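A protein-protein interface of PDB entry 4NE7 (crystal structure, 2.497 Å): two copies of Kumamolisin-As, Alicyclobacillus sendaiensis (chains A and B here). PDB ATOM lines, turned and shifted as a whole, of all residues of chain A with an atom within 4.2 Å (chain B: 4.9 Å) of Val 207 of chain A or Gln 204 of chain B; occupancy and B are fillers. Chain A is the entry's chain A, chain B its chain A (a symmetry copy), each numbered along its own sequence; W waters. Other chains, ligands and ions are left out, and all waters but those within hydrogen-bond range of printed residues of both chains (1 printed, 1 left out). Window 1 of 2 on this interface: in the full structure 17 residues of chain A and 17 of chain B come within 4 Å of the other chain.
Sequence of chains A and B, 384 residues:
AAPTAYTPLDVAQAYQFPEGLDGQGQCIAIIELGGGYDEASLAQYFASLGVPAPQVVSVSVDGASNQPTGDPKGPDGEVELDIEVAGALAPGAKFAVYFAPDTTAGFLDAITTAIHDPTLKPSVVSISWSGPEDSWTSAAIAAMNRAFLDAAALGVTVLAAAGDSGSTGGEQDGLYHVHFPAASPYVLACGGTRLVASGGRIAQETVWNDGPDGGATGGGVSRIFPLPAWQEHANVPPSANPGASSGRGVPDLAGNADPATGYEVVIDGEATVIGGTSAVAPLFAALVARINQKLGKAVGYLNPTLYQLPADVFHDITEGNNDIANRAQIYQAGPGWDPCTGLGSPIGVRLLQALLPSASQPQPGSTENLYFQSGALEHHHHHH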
ATOM      1  N   THR A 206      23.273  -7.211   8.139  1.00  0.00           N
ATOM      2  CA  THR A 206      24.084  -6.051   7.787  1.00  0.00           C
ATOM      3  C   THR A 206      23.600  -5.369   6.510  1.00  0.00           C
ATOM      4  O   THR A 206      22.789  -5.920   5.769  1.00  0.00           O
ATOM      5  CB  THR A 206      25.558  -6.441   7.605  1.00  0.00           C
ATOM      6  OG1 THR A 206      25.663  -7.453   6.592  1.00  0.00           O
ATOM      7  CG2 THR A 206      26.137  -6.969   8.912  1.00  0.00           C
ATOM      8  N   VAL A 207      24.108  -4.165   6.266  1.00  0.00           N
ATOM      9  CA  VAL A 207      23.797  -3.420   5.052  1.00  0.00           C
ATOM     10  C   VAL A 207      24.212  -4.208   3.818  1.00  0.00           C
ATOM     11  O   VAL A 207      25.336  -4.703   3.741  1.00  0.00           O
ATOM     12  CB  VAL A 207      24.515  -2.059   5.040  1.00  0.00           C
ATOM     13  CG1 VAL A 207      24.220  -1.311   3.751  1.00  0.00           C
ATOM     14  CG2 VAL A 207      24.101  -1.236   6.250  1.00  0.00           C
ATOM     15  N   TRP A 208      23.301  -4.336   2.858  1.00  0.00           N
ATOM     16  CA  TRP A 208      23.619  -5.017   1.612  1.00  0.00           C
ATOM     17  C   TRP A 208      24.547  -4.162   0.762  1.00  0.00           C
ATOM     18  O   TRP A 208      24.216  -3.029   0.413  1.00  0.00           O
ATOM     19  CB  TRP A 208      22.352  -5.349   0.830  1.00  0.00           C
ATOM     20  CG  TRP A 208      22.630  -5.867  -0.547  1.00  0.00           C
ATOM     21  CD1 TRP A 208      23.509  -6.848  -0.887  1.00  0.00           C
ATOM     22  CD2 TRP A 208      22.010  -5.441  -1.768  1.00  0.00           C
ATOM     23  NE1 TRP A 208      23.481  -7.060  -2.245  1.00  0.00           N
ATOM     24  CE2 TRP A 208      22.569  -6.209  -2.808  1.00  0.00           C
ATOM     25  CE3 TRP A 208      21.037  -4.487  -2.080  1.00  0.00           C
ATOM     26  CZ2 TRP A 208      22.188  -6.050  -4.141  1.00  0.00           C
ATOM     27  CZ3 TRP A 208      20.661  -4.331  -3.404  1.00  0.00           C
ATOM     28  CH2 TRP A 208      21.236  -5.107  -4.418  1.00  0.00           C
ATOM     29  N   ASN A 209      25.709  -4.713   0.433  1.00  0.00           N
ATOM     30  CA  ASN A 209      26.713  -3.992  -0.332  1.00  0.00           C
ATOM     31  C   ASN A 209      27.691  -4.970  -0.972  1.00  0.00           C
ATOM     32  O   ASN A 209      28.643  -5.419  -0.334  1.00  0.00           O
ATOM     33  CB  ASN A 209      27.456  -3.006   0.576  1.00  0.00           C
ATOM     34  CG  ASN A 209      28.307  -2.012  -0.199  1.00  0.00           C
ATOM     35  OD1 ASN A 209      28.808  -2.309  -1.283  1.00  0.00           O
ATOM     36  ND2 ASN A 209      28.477  -0.820   0.365  1.00  0.00           N
ATOM     37  N   THR A 217      22.429  -1.453  -1.490  1.00  0.00           N
ATOM     38  CA  THR A 217      21.155  -0.804  -1.205  1.00  0.00           C
ATOM     39  C   THR A 217      21.217   0.704  -1.439  1.00  0.00           C
ATOM     40  O   THR A 217      22.190   1.366  -1.080  1.00  0.00           O
ATOM     41  CB  THR A 217      20.661  -1.093   0.234  1.00  0.00           C
ATOM     42  OG1 THR A 217      19.410  -0.433   0.454  1.00  0.00           O
ATOM     43  CG2 THR A 217      21.661  -0.611   1.266  1.00  0.00           C
ATOM     44  N   ILE A 317      19.881  -2.113  12.202  1.00  0.00           N
ATOM     45  CA  ILE A 317      21.117  -2.464  11.513  1.00  0.00           C
ATOM     46  C   ILE A 317      22.154  -1.390  11.816  1.00  0.00           C
ATOM     47  O   ILE A 317      21.900  -0.200  11.625  1.00  0.00           O
ATOM     48  CB  ILE A 317      20.934  -2.587   9.987  1.00  0.00           C
ATOM     49  CG1 ILE A 317      20.274  -3.919   9.617  1.00  0.00           C
ATOM     50  CG2 ILE A 317      22.279  -2.492   9.286  1.00  0.00           C
ATOM     51  CD1 ILE A 317      18.780  -3.956   9.816  1.00  0.00           C
ATOM     52  N   GLU A 319      25.756  -2.082  11.173  1.00  0.00           N
ATOM     53  CA  GLU A 319      27.020  -2.430  10.532  1.00  0.00           C
ATOM     54  C   GLU A 319      26.932  -2.427   9.005  1.00  0.00           C
ATOM     55  O   GLU A 319      26.032  -3.036   8.419  1.00  0.00           O
ATOM     56  CB  GLU A 319      27.514  -3.791  11.033  1.00  0.00           C
ATOM     57  CG  GLU A 319      28.877  -4.203  10.498  1.00  0.00           C
ATOM     58  CD  GLU A 319      30.023  -3.417  11.114  1.00  0.00           C
ATOM     59  OE1 GLU A 319      29.801  -2.724  12.130  1.00  0.00           O
ATOM     60  OE2 GLU A 319      31.151  -3.499  10.581  1.00  0.00           O
ATOM     61  N   GLY A 320      27.883  -1.749   8.369  1.00  0.00           N
ATOM     62  CA  GLY A 320      27.930  -1.668   6.920  1.00  0.00           C
ATOM     63  C   GLY A 320      27.752  -0.255   6.394  1.00  0.00           C
ATOM     64  O   GLY A 320      27.392   0.654   7.143  1.00  0.00           O
ATOM     65  N   ASN A 321      28.004  -0.071   5.100  1.00  0.00           N
ATOM     66  CA  ASN A 321      27.854   1.235   4.464  1.00  0.00           C
ATOM     67  C   ASN A 321      27.248   1.146   3.063  1.00  0.00           C
ATOM     68  O   ASN A 321      27.221   0.071   2.458  1.00  0.00           O
ATOM     69  CB  ASN A 321      29.195   1.975   4.415  1.00  0.00           C
ATOM     70  CG  ASN A 321      30.230   1.251   3.578  1.00  0.00           C
ATOM     71  OD1 ASN A 321      30.183   1.279   2.347  1.00  0.00           O
ATOM     72  ND2 ASN A 321      31.178   0.599   4.242  1.00  0.00           N
ATOM     73  N   ASN A 322      26.771   2.288   2.563  1.00  0.00           N
ATOM     74  CA  ASN A 322      26.105   2.382   1.261  1.00  0.00           C
ATOM     75  C   ASN A 322      27.065   2.582   0.097  1.00  0.00           C
ATOM     76  O   ASN A 322      26.676   2.471  -1.066  1.00  0.00           O
ATOM     77  CB  ASN A 322      25.104   3.543   1.257  1.00  0.00           C
ATOM     78  CG  ASN A 322      23.681   3.079   1.077  1.00  0.00           C
ATOM     79  OD1 ASN A 322      23.284   2.054   1.623  1.00  0.00           O
ATOM     80  ND2 ASN A 322      22.907   3.823   0.299  1.00  0.00           N
ATOM     81  N   ALA A 333      25.749   2.979   8.207  1.00  0.00           N
ATOM     82  CA  ALA A 333      24.725   2.557   9.155  1.00  0.00           C
ATOM     83  C   ALA A 333      25.222   2.743  10.577  1.00  0.00           C
ATOM     84  O   ALA A 333      26.426   2.764  10.827  1.00  0.00           O
ATOM     85  CB  ALA A 333      24.334   1.111   8.923  1.00  0.00           C
ATOM     86  N   CYS A 340      21.051   3.988   5.204  1.00  0.00           N
ATOM     87  CA  CYS A 340      21.326   2.732   4.514  1.00  0.00           C
ATOM     88  C   CYS A 340      20.168   1.761   4.683  1.00  0.00           C
ATOM     89  O   CYS A 340      19.813   1.032   3.758  1.00  0.00           O
ATOM     90  CB  CYS A 340      22.595   2.080   5.064  1.00  0.00           C
ATOM     91  SG  CYS A 340      24.018   3.169   5.208  1.00  0.00           S
ATOM     92  N   THR A 341      19.589   1.749   5.878  1.00  0.00           N
ATOM     93  CA  THR A 341      18.616   0.730   6.243  1.00  0.00           C
ATOM     94  C   THR A 341      17.418   1.320   6.980  1.00  0.00           C
ATOM     95  O   THR A 341      16.526   0.590   7.412  1.00  0.00           O
ATOM     96  CB  THR A 341      19.265  -0.348   7.129  1.00  0.00           C
ATOM     97  OG1 THR A 341      19.901   0.277   8.250  1.00  0.00           O
ATOM     98  CG2 THR A 341      20.307  -1.142   6.342  1.00  0.00           C
ATOM     99  N   ARG B 194      34.253 -12.240  11.178  1.00  0.00           N
ATOM    100  CA  ARG B 194      34.146 -12.357   9.731  1.00  0.00           C
ATOM    101  C   ARG B 194      34.403 -10.982   9.133  1.00  0.00           C
ATOM    102  O   ARG B 194      33.661 -10.036   9.395  1.00  0.00           O
ATOM    103  CB  ARG B 194      32.763 -12.865   9.327  1.00  0.00           C
ATOM    104  CG  ARG B 194      32.580 -13.047   7.833  1.00  0.00           C
ATOM    105  CD  ARG B 194      31.176 -13.537   7.521  1.00  0.00           C
ATOM    106  NE  ARG B 194      30.949 -13.699   6.089  1.00  0.00           N
ATOM    107  CZ  ARG B 194      30.599 -12.705   5.281  1.00  0.00           C
ATOM    108  NH1 ARG B 194      30.447 -11.484   5.772  1.00  0.00           N
ATOM    109  NH2 ARG B 194      30.409 -12.927   3.987  1.00  0.00           N
ATOM    110  N   LEU B 195      35.462 -10.868   8.344  1.00  0.00           N
ATOM    111  CA  LEU B 195      35.889  -9.570   7.840  1.00  0.00           C
ATOM    112  C   LEU B 195      35.548  -9.371   6.370  1.00  0.00           C
ATOM    113  O   LEU B 195      35.894 -10.196   5.522  1.00  0.00           O
ATOM    114  CB  LEU B 195      37.392  -9.389   8.045  1.00  0.00           C
ATOM    115  CG  LEU B 195      37.979  -8.066   7.552  1.00  0.00           C
ATOM    116  CD1 LEU B 195      37.549  -6.910   8.449  1.00  0.00           C
ATOM    117  CD2 LEU B 195      39.491  -8.158   7.470  1.00  0.00           C
ATOM    118  N   VAL B 196      34.861  -8.272   6.081  1.00  0.00           N
ATOM    119  CA  VAL B 196      34.651  -7.831   4.708  1.00  0.00           C
ATOM    120  C   VAL B 196      35.354  -6.491   4.512  1.00  0.00           C
ATOM    121  O   VAL B 196      34.906  -5.456   5.010  1.00  0.00           O
ATOM    122  CB  VAL B 196      33.154  -7.700   4.369  1.00  0.00           C
ATOM    123  CG1 VAL B 196      32.969  -7.161   2.960  1.00  0.00           C
ATOM    124  CG2 VAL B 196      32.464  -9.042   4.514  1.00  0.00           C
ATOM    125  N   ILE B 202      37.512  -1.242   6.209  1.00  0.00           N
ATOM    126  CA  ILE B 202      36.549  -2.236   6.654  1.00  0.00           C
ATOM    127  C   ILE B 202      35.138  -1.876   6.191  1.00  0.00           C
ATOM    128  O   ILE B 202      34.557  -0.889   6.644  1.00  0.00           O
ATOM    129  CB  ILE B 202      36.568  -2.381   8.190  1.00  0.00           C
ATOM    130  CG1 ILE B 202      37.943  -2.854   8.659  1.00  0.00           C
ATOM    131  CG2 ILE B 202      35.490  -3.347   8.645  1.00  0.00           C
ATOM    132  CD1 ILE B 202      38.052  -3.038  10.159  1.00  0.00           C
ATOM    133  N   ALA B 203      34.598  -2.673   5.276  1.00  0.00           N
ATOM    134  CA  ALA B 203      33.222  -2.496   4.833  1.00  0.00           C
ATOM    135  C   ALA B 203      32.284  -2.912   5.959  1.00  0.00           C
ATOM    136  O   ALA B 203      31.422  -2.144   6.381  1.00  0.00           O
ATOM    137  CB  ALA B 203      32.954  -3.314   3.581  1.00  0.00           C
ATOM    138  N   GLN B 204      32.456  -4.141   6.440  1.00  0.00           N
ATOM    139  CA  GLN B 204      31.749  -4.596   7.629  1.00  0.00           C
ATOM    140  C   GLN B 204      32.485  -5.732   8.326  1.00  0.00           C
ATOM    141  O   GLN B 204      33.156  -6.542   7.683  1.00  0.00           O
ATOM    142  CB  GLN B 204      30.309  -4.999   7.302  1.00  0.00           C
ATOM    143  CG  GLN B 204      30.162  -6.256   6.476  1.00  0.00           C
ATOM    144  CD  GLN B 204      28.737  -6.462   5.989  1.00  0.00           C
ATOM    145  OE1 GLN B 204      28.114  -5.544   5.446  1.00  0.00           O
ATOM    146  NE2 GLN B 204      28.218  -7.676   6.169  1.00  0.00           N
ATOM    147  N   GLU B 205      32.364  -5.779   9.648  1.00  0.00           N
ATOM    148  CA  GLU B 205      32.979  -6.849  10.424  1.00  0.00           C
ATOM    149  C   GLU B 205      32.009  -7.377  11.473  1.00  0.00           C
ATOM    150  O   GLU B 205      31.468  -6.613  12.274  1.00  0.00           O
ATOM    151  CB  GLU B 205      34.273  -6.367  11.082  1.00  0.00           C
ATOM    152  CG  GLU B 205      35.213  -7.492  11.475  1.00  0.00           C
ATOM    153  CD  GLU B 205      36.477  -6.996  12.156  1.00  0.00           C
ATOM    154  OE1 GLU B 205      36.574  -5.779  12.433  1.00  0.00           O
ATOM    155  OE2 GLU B 205      37.372  -7.831  12.412  1.00  0.00           O
ATOM    156  N   THR B 206      31.780  -8.685  11.455  1.00  0.00           N
ATOM    157  CA  THR B 206      30.840  -9.304  12.381  1.00  0.00           C
ATOM    158  C   THR B 206      31.446 -10.496  13.116  1.00  0.00           C
ATOM    159  O   THR B 206      32.509 -10.992  12.746  1.00  0.00           O
ATOM    160  CB  THR B 206      29.572  -9.773  11.651  1.00  0.00           C
ATOM    161  OG1 THR B 206      29.932 -10.694  10.611  1.00  0.00           O
ATOM    162  CG2 THR B 206      28.834  -8.585  11.045  1.00  0.00           C
HETATM  163  O   HOH W   1      30.534  -0.691   8.725  1.00  0.00           O
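Thr 206 of chain A touches its own counterpart, Thr 206 of chain B.
1 position is printed for both chains.
N of Ala 333 of chain A is in hydrogen-bond range of O of Gly 320 of chain A, at 3.0 Å.
N of Val 196 of chain B is in hydrogen-bond range of O of Gln 204 of chain B, 2.9 Å away.
The backbone carbonyl oxygen of Asn 321 of chain A is in hydrogen-bond range of the side-chain amide nitrogen of Asn 209 of chain A.
O of Val 196 of chain B sits at hydrogen-bond distance from N of Ala 203 of chain B.
The backbone NH (N) of Arg 194 of chain B is in hydrogen-bond range of the backbone carbonyl oxygen (O) of Thr 206 of chain B, at 2.7 Å.
The backbone carbonyl oxygen (O) of Glu 319 of chain A sits at hydrogen-bond distance from the backbone NH (N) of Val 207 of chain A, at 3.1 Å.
Water W1 lies within hydrogen-bond range of the backbone NH (N) of Gly 320 of chain A (2.9 Å) and the backbone carbonyl oxygen (O) of Ala 203 of chain B (2.9 Å).
CG2 of Thr 206 of chain A touches CG2 of Thr 206 of chain B (3.8 Å).
Gln 204 of chain B touches Glu 319 of chain A.
Ala 203 of chain B touches Gly 320 of chain A.
O of Val 207 of chain A sits close to OE1 of Gln 204 of chain B (3.4 Å).
The side-chain amide nitrogen of Gln 204 of chain B lies within hydrogen-bond range of the side-chain hydroxyl of Thr 206 of chain A (2.6 Å).
ND2 of Asn 321 of chain A is in hydrogen-bond range of O of Ala 203 of chain B.
The side-chain carboxylate of Glu 319 of chain A sits close to the backbone NH of Glu 205 of chain B (2.7 Å).
Printed residues of chain B that touch a printed residue of chain A: Ala 203, Gln 204, Glu 205 and Thr 206.
Along chain B the printed residues that touch a printed residue of chain A span positions 203 to 206.
Among the printed residues, 7 pairs touch across the chains.
Among the printed residues, no Asp or Glu carboxylate lies within 4 Å of a Lys or Arg side-chain nitrogen of the other chain.
Val 207 of chain A touches just one residue of chain B: Gln 204 (3.4 Å).
Printed residues of chain A within 4 Å of Glu 205 of chain B: Glu 319.
Printed residues of chain B within 4 Å of Gly 320 of chain A: Ala 203.
Thr 217 of chain A touches none of the printed residues of chain B.
Cys 340 of chain A touches none of the printed residues of chain B.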
